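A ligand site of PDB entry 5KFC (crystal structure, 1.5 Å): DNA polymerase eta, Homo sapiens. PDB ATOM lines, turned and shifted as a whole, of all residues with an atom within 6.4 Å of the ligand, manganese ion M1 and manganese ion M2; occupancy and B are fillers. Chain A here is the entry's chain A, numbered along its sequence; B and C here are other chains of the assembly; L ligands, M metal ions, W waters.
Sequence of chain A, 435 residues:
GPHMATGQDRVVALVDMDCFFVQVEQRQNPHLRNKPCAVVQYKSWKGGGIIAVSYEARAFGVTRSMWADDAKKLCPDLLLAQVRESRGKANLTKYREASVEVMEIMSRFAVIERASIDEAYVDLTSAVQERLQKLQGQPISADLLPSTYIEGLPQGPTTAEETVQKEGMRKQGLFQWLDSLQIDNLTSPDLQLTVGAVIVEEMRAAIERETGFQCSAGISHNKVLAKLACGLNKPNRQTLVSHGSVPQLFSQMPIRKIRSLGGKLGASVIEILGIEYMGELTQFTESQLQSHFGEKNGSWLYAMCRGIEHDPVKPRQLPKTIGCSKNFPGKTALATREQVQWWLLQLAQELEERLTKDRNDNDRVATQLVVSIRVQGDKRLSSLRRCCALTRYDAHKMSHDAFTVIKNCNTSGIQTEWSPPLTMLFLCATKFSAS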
ATOM      1  N   ASP A  16      19.147  24.211  26.924  1.00  0.00           N
ATOM      2  CA  ASP A  16      19.505  22.813  27.095  1.00  0.00           C
ATOM      3  C   ASP A  16      18.916  22.265  28.380  1.00  0.00           C
ATOM      4  O   ASP A  16      19.123  22.826  29.453  1.00  0.00           O
ATOM      5  CB  ASP A  16      21.019  22.624  27.100  1.00  0.00           C
ATOM      6  CG  ASP A  16      21.414  21.197  27.338  1.00  0.00           C
ATOM      7  OD1 ASP A  16      21.516  20.807  28.511  1.00  0.00           O
ATOM      8  OD2 ASP A  16      21.613  20.460  26.347  1.00  0.00           O
ATOM      9  N   MET A  17      18.184  21.165  28.281  1.00  0.00           N
ATOM     10  CA  MET A  17      17.499  20.630  29.449  1.00  0.00           C
ATOM     11  C   MET A  17      18.476  20.088  30.498  1.00  0.00           C
ATOM     12  O   MET A  17      19.480  19.504  30.153  1.00  0.00           O
ATOM     13  CB  MET A  17      16.517  19.526  29.035  1.00  0.00           C
ATOM     14  CG  MET A  17      15.542  19.958  27.948  1.00  0.00           C
ATOM     15  SD  MET A  17      14.583  21.439  28.324  1.00  0.00           S
ATOM     16  CE  MET A  17      13.607  20.877  29.666  1.00  0.00           C
ATOM     17  N   ASP A  18      18.170  20.296  31.780  1.00  0.00           N
ATOM     18  CA  ASP A  18      19.026  19.733  32.832  1.00  0.00           C
ATOM     19  C   ASP A  18      18.775  18.238  33.008  1.00  0.00           C
ATOM     20  O   ASP A  18      17.603  17.809  33.121  1.00  0.00           O
ATOM     21  CB  ASP A  18      18.745  20.391  34.180  1.00  0.00           C
ATOM     22  CG  ASP A  18      19.019  21.886  34.176  1.00  0.00           C
ATOM     23  OD1 ASP A  18      19.849  22.365  33.394  1.00  0.00           O
ATOM     24  OD2 ASP A  18      18.368  22.566  34.981  1.00  0.00           O
ATOM     25  N   CYS A  19      19.866  17.471  33.005  1.00  0.00           N
ATOM     26  CA  CYS A  19      19.861  16.002  33.180  1.00  0.00           C
ATOM     27  C   CYS A  19      18.570  15.412  32.597  1.00  0.00           C
ATOM     28  O   CYS A  19      17.765  14.825  33.310  1.00  0.00           O
ATOM     29  CB  CYS A  19      20.061  15.582  34.653  1.00  0.00           C
ATOM     30  SG  CYS A  19      19.023  16.319  35.933  1.00  0.00           S
ATOM     31  N   PHE A  20      18.398  15.578  31.291  1.00  0.00           N
ATOM     32  CA  PHE A  20      17.076  15.482  30.689  1.00  0.00           C
ATOM     33  C   PHE A  20      16.350  14.155  30.934  1.00  0.00           C
ATOM     34  O   PHE A  20      15.231  14.182  31.433  1.00  0.00           O
ATOM     35  CB  PHE A  20      17.159  15.740  29.165  1.00  0.00           C
ATOM     36  CG  PHE A  20      15.816  15.758  28.468  1.00  0.00           C
ATOM     37  CD1 PHE A  20      14.748  16.487  28.997  1.00  0.00           C
ATOM     38  CD2 PHE A  20      15.618  15.058  27.288  1.00  0.00           C
ATOM     39  CE1 PHE A  20      13.512  16.521  28.335  1.00  0.00           C
ATOM     40  CE2 PHE A  20      14.379  15.093  26.643  1.00  0.00           C
ATOM     41  CZ  PHE A  20      13.338  15.828  27.178  1.00  0.00           C
ATOM     42  N   PHE A  21      16.961  13.020  30.616  1.00  0.00           N
ATOM     43  CA  PHE A  21      16.217  11.771  30.766  1.00  0.00           C
ATOM     44  C   PHE A  21      15.852  11.529  32.240  1.00  0.00           C
ATOM     45  O   PHE A  21      14.828  10.926  32.538  1.00  0.00           O
ATOM     46  CB  PHE A  21      16.981  10.552  30.235  1.00  0.00           C
ATOM     47  CG  PHE A  21      17.138  10.481  28.745  1.00  0.00           C
ATOM     48  CD1 PHE A  21      16.835  11.573  27.914  1.00  0.00           C
ATOM     49  CD2 PHE A  21      17.606   9.314  28.160  1.00  0.00           C
ATOM     50  CE1 PHE A  21      16.997  11.473  26.533  1.00  0.00           C
ATOM     51  CE2 PHE A  21      17.761   9.209  26.784  1.00  0.00           C
ATOM     52  CZ  PHE A  21      17.471  10.296  25.967  1.00  0.00           C
ATOM     53  N   VAL A  22      16.708  11.989  33.156  1.00  0.00           N
ATOM     54  CA  VAL A  22      16.395  11.859  34.581  1.00  0.00           C
ATOM     55  C   VAL A  22      15.160  12.679  34.929  1.00  0.00           C
ATOM     56  O   VAL A  22      14.245  12.187  35.603  1.00  0.00           O
ATOM     57  CB  VAL A  22      17.600  12.285  35.456  1.00  0.00           C
ATOM     58  CG1 VAL A  22      17.162  12.528  36.903  1.00  0.00           C
ATOM     59  CG2 VAL A  22      18.695  11.222  35.396  1.00  0.00           C
ATOM     60  N   GLN A  41      20.406   1.856  30.693  1.00  0.00           N
ATOM     61  CA  GLN A  41      19.814   0.969  29.686  1.00  0.00           C
ATOM     62  C   GLN A  41      20.456  -0.404  29.782  1.00  0.00           C
ATOM     63  O   GLN A  41      21.679  -0.552  29.929  1.00  0.00           O
ATOM     64  CB  GLN A  41      19.898   1.557  28.265  1.00  0.00           C
ATOM     65  CG  GLN A  41      21.240   1.995  27.763  1.00  0.00           C
ATOM     66  CD  GLN A  41      21.143   2.769  26.435  1.00  0.00           C
ATOM     67  OE1 GLN A  41      20.051   3.034  25.899  1.00  0.00           O
ATOM     68  NE2 GLN A  41      22.296   3.119  25.905  1.00  0.00           N
ATOM     69  N   ILE A  51      23.156   6.493  31.223  1.00  0.00           N
ATOM     70  CA  ILE A  51      23.160   7.499  30.154  1.00  0.00           C
ATOM     71  C   ILE A  51      22.706   8.882  30.619  1.00  0.00           C
ATOM     72  O   ILE A  51      22.823   9.837  29.871  1.00  0.00           O
ATOM     73  CB  ILE A  51      22.286   7.065  28.949  1.00  0.00           C
ATOM     74  CG1 ILE A  51      20.823   6.833  29.350  1.00  0.00           C
ATOM     75  CG2 ILE A  51      22.899   5.834  28.273  1.00  0.00           C
ATOM     76  CD1 ILE A  51      19.894   6.610  28.152  1.00  0.00           C
ATOM     77  N   ALA A  52      22.241   9.009  31.862  1.00  0.00           N
ATOM     78  CA  ALA A  52      21.888  10.328  32.410  1.00  0.00           C
ATOM     79  C   ALA A  52      21.959  10.273  33.934  1.00  0.00           C
ATOM     80  O   ALA A  52      21.637   9.235  34.521  1.00  0.00           O
ATOM     81  CB  ALA A  52      20.479  10.771  31.960  1.00  0.00           C
ATOM     82  N   VAL A  53      22.345  11.384  34.566  1.00  0.00           N
ATOM     83  CA  VAL A  53      22.674  11.415  36.004  1.00  0.00           C
ATOM     84  C   VAL A  53      22.148  12.679  36.657  1.00  0.00           C
ATOM     85  O   VAL A  53      22.442  13.781  36.169  1.00  0.00           O
ATOM     86  CB  VAL A  53      24.209  11.350  36.235  1.00  0.00           C
ATOM     87  CG1 VAL A  53      24.529  11.211  37.722  1.00  0.00           C
ATOM     88  CG2 VAL A  53      24.829  10.194  35.482  1.00  0.00           C
ATOM     89  N   TYR A  55      21.883  15.732  39.406  1.00  0.00           N
ATOM     90  CA  TYR A  55      22.969  16.513  39.981  1.00  0.00           C
ATOM     91  C   TYR A  55      23.311  16.029  41.379  1.00  0.00           C
ATOM     92  O   TYR A  55      24.484  16.064  41.778  1.00  0.00           O
ATOM     93  CB  TYR A  55      22.615  18.008  39.933  1.00  0.00           C
ATOM     94  CG  TYR A  55      22.865  18.549  38.544  1.00  0.00           C
ATOM     95  CD1 TYR A  55      21.931  18.371  37.528  1.00  0.00           C
ATOM     96  CD2 TYR A  55      24.066  19.179  38.225  1.00  0.00           C
ATOM     97  CE1 TYR A  55      22.173  18.829  36.228  1.00  0.00           C
ATOM     98  CE2 TYR A  55      24.312  19.657  36.955  1.00  0.00           C
ATOM     99  CZ  TYR A  55      23.377  19.471  35.951  1.00  0.00           C
ATOM    100  OH  TYR A  55      23.622  19.927  34.675  1.00  0.00           O
ATOM    101  N   ARG A  58      25.667  13.243  40.755  1.00  0.00           N
ATOM    102  CA  ARG A  58      26.957  13.705  40.265  1.00  0.00           C
ATOM    103  C   ARG A  58      27.882  14.087  41.422  1.00  0.00           C
ATOM    104  O   ARG A  58      29.095  13.947  41.296  1.00  0.00           O
ATOM    105  CB  ARG A  58      26.811  14.900  39.318  1.00  0.00           C
ATOM    106  CG  ARG A  58      26.018  14.569  38.076  1.00  0.00           C
ATOM    107  CD  ARG A  58      25.921  15.749  37.122  1.00  0.00           C
ATOM    108  NE  ARG A  58      24.876  15.479  36.131  1.00  0.00           N
ATOM    109  CZ  ARG A  58      24.663  16.190  35.033  1.00  0.00           C
ATOM    110  NH1 ARG A  58      25.427  17.238  34.762  1.00  0.00           N
ATOM    111  NH2 ARG A  58      23.669  15.837  34.202  1.00  0.00           N
ATOM    112  N   ARG A  64      27.830   9.630  33.256  1.00  0.00           N
ATOM    113  CA  ARG A  64      27.447   8.915  32.054  1.00  0.00           C
ATOM    114  C   ARG A  64      28.537   7.907  31.648  1.00  0.00           C
ATOM    115  O   ARG A  64      29.711   8.110  31.937  1.00  0.00           O
ATOM    116  CB  ARG A  64      27.189   9.924  30.927  1.00  0.00           C
ATOM    117  CG  ARG A  64      26.975   9.358  29.545  1.00  0.00           C
ATOM    118  CD  ARG A  64      26.566  10.473  28.596  1.00  0.00           C
ATOM    119  NE  ARG A  64      25.285  11.005  29.042  1.00  0.00           N
ATOM    120  CZ  ARG A  64      24.987  12.297  29.153  1.00  0.00           C
ATOM    121  NH1 ARG A  64      25.866  13.252  28.821  1.00  0.00           N
ATOM    122  NH2 ARG A  64      23.787  12.641  29.591  1.00  0.00           N
ATOM    123  N   LEU A  92      13.610   4.607  22.842  1.00  0.00           N
ATOM    124  CA  LEU A  92      13.748   5.939  23.432  1.00  0.00           C
ATOM    125  C   LEU A  92      12.522   6.841  23.201  1.00  0.00           C
ATOM    126  O   LEU A  92      12.619   8.058  23.342  1.00  0.00           O
ATOM    127  CB  LEU A  92      14.992   6.633  22.878  1.00  0.00           C
ATOM    128  CG  LEU A  92      16.299   5.858  23.012  1.00  0.00           C
ATOM    129  CD1 LEU A  92      17.409   6.595  22.274  1.00  0.00           C
ATOM    130  CD2 LEU A  92      16.661   5.698  24.496  1.00  0.00           C
ATOM    131  N   SER A 116      19.769  18.703  19.404  1.00  0.00           N
ATOM    132  CA  SER A 116      19.815  17.384  20.018  1.00  0.00           C
ATOM    133  C   SER A 116      18.448  17.040  20.572  1.00  0.00           C
ATOM    134  O   SER A 116      17.522  17.841  20.498  1.00  0.00           O
ATOM    135  CB  SER A 116      20.853  17.316  21.152  1.00  0.00           C
ATOM    136  OG  SER A 116      20.343  17.844  22.358  1.00  0.00           O
ATOM    137  N   ILE A 117      18.334  15.876  21.183  1.00  0.00           N
ATOM    138  CA  ILE A 117      17.078  15.509  21.797  1.00  0.00           C
ATOM    139  C   ILE A 117      16.700  16.482  22.921  1.00  0.00           C
ATOM    140  O   ILE A 117      15.534  16.597  23.272  1.00  0.00           O
ATOM    141  CB  ILE A 117      17.125  14.052  22.339  1.00  0.00           C
ATOM    142  CG1 ILE A 117      15.706  13.511  22.549  1.00  0.00           C
ATOM    143  CG2 ILE A 117      17.971  13.949  23.614  1.00  0.00           C
ATOM    144  CD1 ILE A 117      15.685  12.002  22.739  1.00  0.00           C
ATOM    145  N   ASP A 118      17.659  17.200  23.505  1.00  0.00           N
ATOM    146  CA  ASP A 118      17.284  18.016  24.645  1.00  0.00           C
ATOM    147  C   ASP A 118      17.760  19.466  24.532  1.00  0.00           C
ATOM    148  O   ASP A 118      17.810  20.191  25.549  1.00  0.00           O
ATOM    149  CB  ASP A 118      17.809  17.397  25.951  1.00  0.00           C
ATOM    150  CG  ASP A 118      19.227  17.817  26.288  1.00  0.00           C
ATOM    151  OD1 ASP A 118      20.081  17.974  25.384  1.00  0.00           O
ATOM    152  OD2 ASP A 118      19.459  18.104  27.497  1.00  0.00           O
ATOM    153  N   GLU A 119      18.080  19.917  23.327  1.00  0.00           N
ATOM    154  CA  GLU A 119      18.474  21.320  23.203  1.00  0.00           C
ATOM    155  C   GLU A 119      18.188  21.911  21.843  1.00  0.00           C
ATOM    156  O   GLU A 119      18.127  21.205  20.829  1.00  0.00           O
ATOM    157  CB  GLU A 119      19.945  21.487  23.521  1.00  0.00           C
ATOM    158  CG  GLU A 119      20.864  21.069  22.432  1.00  0.00           C
ATOM    159  CD  GLU A 119      22.203  20.651  22.978  1.00  0.00           C
ATOM    160  OE1 GLU A 119      23.155  21.437  22.896  1.00  0.00           O
ATOM    161  OE2 GLU A 119      22.290  19.522  23.508  1.00  0.00           O
ATOM    162  N   SER A 216      18.805  24.950  31.449  1.00  0.00           N
ATOM    163  CA  SER A 216      19.743  26.056  31.481  1.00  0.00           C
ATOM    164  C   SER A 216      19.769  26.711  30.118  1.00  0.00           C
ATOM    165  O   SER A 216      19.230  26.176  29.149  1.00  0.00           O
ATOM    166  CB  SER A 216      21.120  25.565  31.889  1.00  0.00           C
ATOM    167  OG  SER A 216      21.069  24.980  33.187  1.00  0.00           O
ATOM    168  N   LYS A 227      26.219  28.179  23.280  1.00  0.00           N
ATOM    169  CA  LYS A 227      26.422  26.836  23.805  1.00  0.00           C
ATOM    170  C   LYS A 227      27.407  26.835  24.979  1.00  0.00           C
ATOM    171  O   LYS A 227      27.170  26.209  26.018  1.00  0.00           O
ATOM    172  CB  LYS A 227      26.929  25.903  22.691  1.00  0.00           C
ATOM    173  CG  LYS A 227      27.207  24.473  23.164  1.00  0.00           C
ATOM    174  CD  LYS A 227      25.992  23.839  23.834  1.00  0.00           C
ATOM    175  CE  LYS A 227      26.261  22.386  24.199  1.00  0.00           C
ATOM    176  NZ  LYS A 227      25.092  21.681  24.793  1.00  0.00           N
ATOM    177  N   LYS A 234      25.088  25.816  34.876  1.00  0.00           N
ATOM    178  CA  LYS A 234      24.083  24.735  35.101  1.00  0.00           C
ATOM    179  C   LYS A 234      24.087  24.222  36.551  1.00  0.00           C
ATOM    180  O   LYS A 234      25.146  24.159  37.098  1.00  0.00           O
ATOM    181  CB  LYS A 234      24.427  23.561  34.199  1.00  0.00           C
ATOM    182  CG  LYS A 234      23.793  23.608  32.859  1.00  0.00           C
ATOM    183  CD  LYS A 234      23.779  22.298  32.047  1.00  0.00           C
ATOM    184  CE  LYS A 234      22.887  22.453  30.760  1.00  0.00           C
ATOM    185  NZ  LYS A 234      21.657  21.678  31.058  1.00  0.00           N
ATOM    186  N   PRO A 235      23.018  23.630  37.081  1.00  0.00           N
ATOM    187  CA  PRO A 235      21.734  23.636  36.397  1.00  0.00           C
ATOM    188  C   PRO A 235      20.775  24.776  36.745  1.00  0.00           C
ATOM    189  O   PRO A 235      21.021  25.490  37.616  1.00  0.00           O
ATOM    190  CB  PRO A 235      21.108  22.327  36.888  1.00  0.00           C
ATOM    191  CG  PRO A 235      21.487  22.232  38.297  1.00  0.00           C
ATOM    192  CD  PRO A 235      22.803  22.850  38.418  1.00  0.00           C
ATOM    193  P    DT B   8      27.338  18.958  21.785  1.00  0.00           P
ATOM    194  OP1  DT B   8      26.829  19.379  20.469  1.00  0.00           O
ATOM    195  OP2  DT B   8      27.678  19.969  22.805  1.00  0.00           O
ATOM    196  O5'  DT B   8      26.314  17.958  22.459  1.00  0.00           O
ATOM    197  C5'  DT B   8      25.049  17.912  21.987  1.00  0.00           C
ATOM    198  C4'  DT B   8      24.298  16.700  22.507  1.00  0.00           C
ATOM    199  O4'  DT B   8      24.757  15.453  21.945  1.00  0.00           O
ATOM    200  C3'  DT B   8      24.181  16.475  24.018  1.00  0.00           C
ATOM    201  O3'  DT B   8      22.837  16.658  24.434  1.00  0.00           O
ATOM    202  C2'  DT B   8      24.682  15.031  24.227  1.00  0.00           C
ATOM    203  C1'  DT B   8      24.491  14.419  22.851  1.00  0.00           C
ATOM    204  N1   DT B   8      25.412  13.280  22.578  1.00  0.00           N
ATOM    205  C2   DT B   8      24.885  12.059  22.236  1.00  0.00           C
ATOM    206  O2   DT B   8      23.703  11.857  22.159  1.00  0.00           O
ATOM    207  N3   DT B   8      25.821  11.069  22.010  1.00  0.00           N
ATOM    208  C4   DT B   8      27.195  11.189  22.072  1.00  0.00           C
ATOM    209  O4   DT B   8      27.947  10.248  21.857  1.00  0.00           O
ATOM    210  C5   DT B   8      27.675  12.505  22.430  1.00  0.00           C
ATOM    211  C7   DT B   8      29.151  12.762  22.529  1.00  0.00           C
ATOM    212  C6   DT B   8      26.773  13.470  22.659  1.00  0.00           C
ATOM    213  P    DT C   3      33.340  -1.208  27.388  1.00  0.00           P
ATOM    214  OP1  DT C   3      34.287  -1.344  26.256  1.00  0.00           O
ATOM    215  OP2  DT C   3      33.824  -1.232  28.783  1.00  0.00           O
ATOM    216  O5'  DT C   3      32.492   0.124  27.159  1.00  0.00           O
ATOM    217  C5'  DT C   3      31.327   0.361  27.926  1.00  0.00           C
ATOM    218  C4'  DT C   3      30.459   1.422  27.274  1.00  0.00           C
ATOM    219  O4'  DT C   3      30.955   2.733  27.630  1.00  0.00           O
ATOM    220  C3'  DT C   3      30.454   1.360  25.737  1.00  0.00           C
ATOM    221  O3'  DT C   3      29.125   1.208  25.260  1.00  0.00           O
ATOM    222  C2'  DT C   3      31.096   2.676  25.303  1.00  0.00           C
ATOM    223  C1'  DT C   3      30.879   3.580  26.511  1.00  0.00           C
ATOM    224  N1   DT C   3      31.924   4.624  26.662  1.00  0.00           N
ATOM    225  C2   DT C   3      31.545   5.944  26.702  1.00  0.00           C
ATOM    226  O2   DT C   3      30.393   6.312  26.618  1.00  0.00           O
ATOM    227  N3   DT C   3      32.582   6.827  26.850  1.00  0.00           N
ATOM    228  C4   DT C   3      33.927   6.539  26.956  1.00  0.00           C
ATOM    229  O4   DT C   3      34.785   7.405  27.089  1.00  0.00           O
ATOM    230  C5   DT C   3      34.252   5.132  26.907  1.00  0.00           C
ATOM    231  C7   DT C   3      35.686   4.682  27.007  1.00  0.00           C
ATOM    232  C6   DT C   3      33.253   4.252  26.756  1.00  0.00           C
ATOM    233  P    DT C   4      28.753  -0.074  24.357  1.00  0.00           P
ATOM    234  OP1  DT C   4      29.012  -1.284  25.175  1.00  0.00           O
ATOM    235  OP2  DT C   4      29.465   0.124  23.072  1.00  0.00           O
ATOM    236  O5'  DT C   4      27.187   0.079  24.045  1.00  0.00           O
ATOM    237  C5'  DT C   4      26.182  -0.424  24.942  1.00  0.00           C
ATOM    238  C4'  DT C   4      24.836   0.195  24.603  1.00  0.00           C
ATOM    239  O4'  DT C   4      24.921   1.612  24.831  1.00  0.00           O
ATOM    240  C3'  DT C   4      24.390   0.030  23.155  1.00  0.00           C
ATOM    241  O3'  DT C   4      22.974  -0.063  23.125  1.00  0.00           O
ATOM    242  C2'  DT C   4      24.893   1.327  22.496  1.00  0.00           C
ATOM    243  C1'  DT C   4      24.644   2.319  23.624  1.00  0.00           C
ATOM    244  N1   DT C   4      25.488   3.521  23.645  1.00  0.00           N
ATOM    245  C2   DT C   4      24.903   4.681  24.057  1.00  0.00           C
ATOM    246  O2   DT C   4      23.712   4.756  24.321  1.00  0.00           O
ATOM    247  N3   DT C   4      25.731   5.761  24.107  1.00  0.00           N
ATOM    248  C4   DT C   4      27.077   5.794  23.840  1.00  0.00           C
ATOM    249  O4   DT C   4      27.730   6.823  23.929  1.00  0.00           O
ATOM    250  C5   DT C   4      27.647   4.526  23.433  1.00  0.00           C
ATOM    251  C7   DT C   4      29.116   4.434  23.101  1.00  0.00           C
ATOM    252  C6   DT C   4      26.840   3.455  23.381  1.00  0.00           C
ATOM    253  P    DA C   5      22.188  -0.256  21.745  1.00  0.00           P
ATOM    254  OP1  DA C   5      21.059  -1.161  22.051  1.00  0.00           O
ATOM    255  OP2  DA C   5      23.144  -0.561  20.673  1.00  0.00           O
ATOM    256  O5'  DA C   5      21.592   1.192  21.456  1.00  0.00           O
ATOM    257  C5'  DA C   5      20.611   1.745  22.316  1.00  0.00           C
ATOM    258  C4'  DA C   5      20.130   3.079  21.783  1.00  0.00           C
ATOM    259  O4'  DA C   5      21.168   4.094  21.957  1.00  0.00           O
ATOM    260  C3'  DA C   5      19.800   3.073  20.286  1.00  0.00           C
ATOM    261  O3'  DA C   5      18.683   3.903  20.075  1.00  0.00           O
ATOM    262  C2'  DA C   5      21.065   3.667  19.669  1.00  0.00           C
ATOM    263  C1'  DA C   5      21.431   4.714  20.705  1.00  0.00           C
ATOM    264  N9   DA C   5      22.813   5.118  20.674  1.00  0.00           N
ATOM    265  C8   DA C   5      23.896   4.337  20.374  1.00  0.00           C
ATOM    266  N7   DA C   5      25.044   4.980  20.457  1.00  0.00           N
ATOM    267  C5   DA C   5      24.682   6.256  20.850  1.00  0.00           C
ATOM    268  C6   DA C   5      25.433   7.410  21.112  1.00  0.00           C
ATOM    269  N6   DA C   5      26.762   7.455  21.012  1.00  0.00           N
ATOM    270  N1   DA C   5      24.770   8.530  21.484  1.00  0.00           N
ATOM    271  C2   DA C   5      23.434   8.480  21.588  1.00  0.00           C
ATOM    272  N3   DA C   5      22.616   7.449  21.368  1.00  0.00           N
ATOM    273  C4   DA C   5      23.318   6.354  20.998  1.00  0.00           C
HETATM  274  P1  LIG L   1      23.125  18.227  31.615  1.00  0.00           P
HETATM  275  O1  LIG L   1      22.837  18.826  30.260  1.00  0.00           O
HETATM  276  O2  LIG L   1      22.324  18.860  32.725  1.00  0.00           O
HETATM  277  O3  LIG L   1      24.621  18.229  31.954  1.00  0.00           O
HETATM  278  P2  LIG L   1      22.018  15.895  30.374  1.00  0.00           P
HETATM  279  O4  LIG L   1      20.805  16.671  29.901  1.00  0.00           O
HETATM  280  O5  LIG L   1      21.650  14.505  30.847  1.00  0.00           O
HETATM  281  O6  LIG L   1      22.711  16.681  31.602  1.00  0.00           O
HETATM  282  P3  LIG L   1      23.088  16.117  27.701  1.00  0.00           P
HETATM  283  O7  LIG L   1      22.530  17.466  27.375  1.00  0.00           O
HETATM  284  O8  LIG L   1      24.526  15.930  27.228  1.00  0.00           O
HETATM  285  O9  LIG L   1      23.143  15.798  29.263  1.00  0.00           O
HETATM  286  O10 LIG L   1      22.228  14.964  27.043  1.00  0.00           O
HETATM  287  C1  LIG L   1      20.828  15.013  27.030  1.00  0.00           C
HETATM  288  C2  LIG L   1      20.245  13.599  27.083  1.00  0.00           C
HETATM  289  O11 LIG L   1      20.689  12.910  25.937  1.00  0.00           O
HETATM  290  C3  LIG L   1      20.702  12.860  28.247  1.00  0.00           C
HETATM  291  O12 LIG L   1      19.846  13.086  29.384  1.00  0.00           O
HETATM  292  C4  LIG L   1      20.696  11.457  27.806  1.00  0.00           C
HETATM  293  C5  LIG L   1      21.012  11.572  26.347  1.00  0.00           C
HETATM  294  N1  LIG L   1      22.386  11.330  26.063  1.00  0.00           N
HETATM  295  C6  LIG L   1      23.414  12.205  26.120  1.00  0.00           C
HETATM  296  N2  LIG L   1      24.556  11.606  25.799  1.00  0.00           N
HETATM  297  C7  LIG L   1      24.288  10.325  25.487  1.00  0.00           C
HETATM  298  C8  LIG L   1      25.041   9.230  25.086  1.00  0.00           C
HETATM  299  N3  LIG L   1      26.451   9.357  24.902  1.00  0.00           N
HETATM  300  N4  LIG L   1      24.431   8.059  24.874  1.00  0.00           N
HETATM  301  C9  LIG L   1      23.102   7.892  25.030  1.00  0.00           C
HETATM  302  N5  LIG L   1      22.337   8.947  25.428  1.00  0.00           N
HETATM  303  C10 LIG L   1      22.909  10.144  25.655  1.00  0.00           C
HETATM  304 MN    MN M   1      22.210  18.654  25.515  1.00  0.00          MN
HETATM  305 MN    MN M   2      21.082  18.693  28.879  1.00  0.00          MN
HETATM  306  O   HOH W   1      24.301  19.182  25.985  1.00  0.00           O
HETATM  307  O   HOH W   2      23.200  13.400  32.785  1.00  0.00           O
HETATM  308  O   HOH W   3      19.835   8.097  24.450  1.00  0.00           O
HETATM  309  O   HOH W   4      21.099  11.498  22.838  1.00  0.00           O
HETATM  310  O   HOH W   5      24.868  19.740  28.704  1.00  0.00           O
HETATM  311  O   HOH W   6      26.373  16.293  31.361  1.00  0.00           O
HETATM  312  O   HOH W   7      21.346  14.674  23.894  1.00  0.00           O
HETATM  313  O   HOH W   8      27.338  12.115  25.830  1.00  0.00           O
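O of Asp 16 lies within hydrogen-bond range of NZ of Lys 234. The side-chain hydroxyl (OG) of Ser 116 is in hydrogen-bond range of the backbone NH (N) of Glu 119 (3.2 Å). The side-chain carboxylate (OE1) of Glu 119 lies within salt-bridge range of the side-chain amino group (NZ) of Lys 227 (2.7 Å). The backbone carbonyl oxygen (O) of Met 17 sits close to the side-chain amino group (NZ) of Lys 234 (3.2 Å). OP2 of DT 8 of chain B is in salt-bridge range of NZ of Lys 227, at 3.7 Å. NH1 of Arg 58 sits at hydrogen-bond distance from OH of Tyr 55, at 3.2 Å. The backbone carbonyl oxygen (O) of Val 53 is in hydrogen-bond range of the guanidinium group (NE) of Arg 58, 3.0 Å away. OD1 of Asp 18 is in hydrogen-bond range of OG of Ser 216, at 2.9 Å.
N3 of DT 8 of chain B lies within hydrogen-bond range of a nitrogen (N3) of the ligand (3.4 Å). OH of Tyr 55 sits at hydrogen-bond distance from O2 of the ligand (2.6 Å). O4 of DT 4 of chain C sits at hydrogen-bond distance from N3 of the ligand (3.0 Å). The backbone NH of Cys 19 sits at hydrogen-bond distance from an oxygen (O2) of the ligand (2.8 Å). An oxygen (O3) of the ligand lies within salt-bridge range of the guanidinium group (NH1) of Arg 58 (3.1 Å). An oxygen (O5) of the ligand is in hydrogen-bond range of the backbone NH (N) of Phe 20 (3.5 Å). NH2 of Arg 64 is in salt-bridge range of O5 of the ligand (3.1 Å). The backbone NH (N) of Phe 21 lies within hydrogen-bond range of an oxygen (O12) of the ligand. The side-chain amino group (NZ) of Lys 234 is in salt-bridge range of an oxygen (O2) of the ligand, at 3.3 Å.
Water W1 lies within hydrogen-bond range of the side-chain amino group of Lys 227 and an oxygen (O8) of the ligand. Water W4 lies within hydrogen-bond range of O2 of DT 8 of chain B and O11 of the ligand.
Manganese ion M2 is bound by OD1 of Asp 16, O of Met 17, OD2 of Asp 118, O1 of the ligand, O4 of the ligand and O7 of the ligand.
Ser 116 touches manganese ion M1. Of the 27 residues printed, 5 come within 4 Å of manganese ion M1. Along chain A the residues within 4 Å of manganese ion M1 span positions 16 to 119.
Manganese ion M1 is bound by OD2 of Asp 16 (2.1 Å), OE2 of Glu 119 (2.2 Å), water W1 (2.2 Å), O7 of the ligand (2.2 Å), OD1 of Asp 118 (2.2 Å) and O3' of DT 8 of chain B (2.4 Å).
NZ of Lys 234 touches manganese ion M2, at 3.7 Å. Of the 27 residues printed, 4 come within 4 Å of manganese ion M2. The nearest printed residue that does not touch manganese ion M2 is Asp 18 (4.4 Å).
N4 of the ligand lies close to N1 of DA 5 of chain C, 3.4 Å away. Asp 18 touches the ligand. Ile 51 touches the ligand. Ala 52 touches the ligand (CB to O12, 3.5 Å). Ile 117 touches the ligand (CG2 to O11, 3.7 Å). Hydrophobic or aromatic side chains that line the ligand: Phe 20, Phe 21, Ile 51, Ala 52, Tyr 55 and Ile 117.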
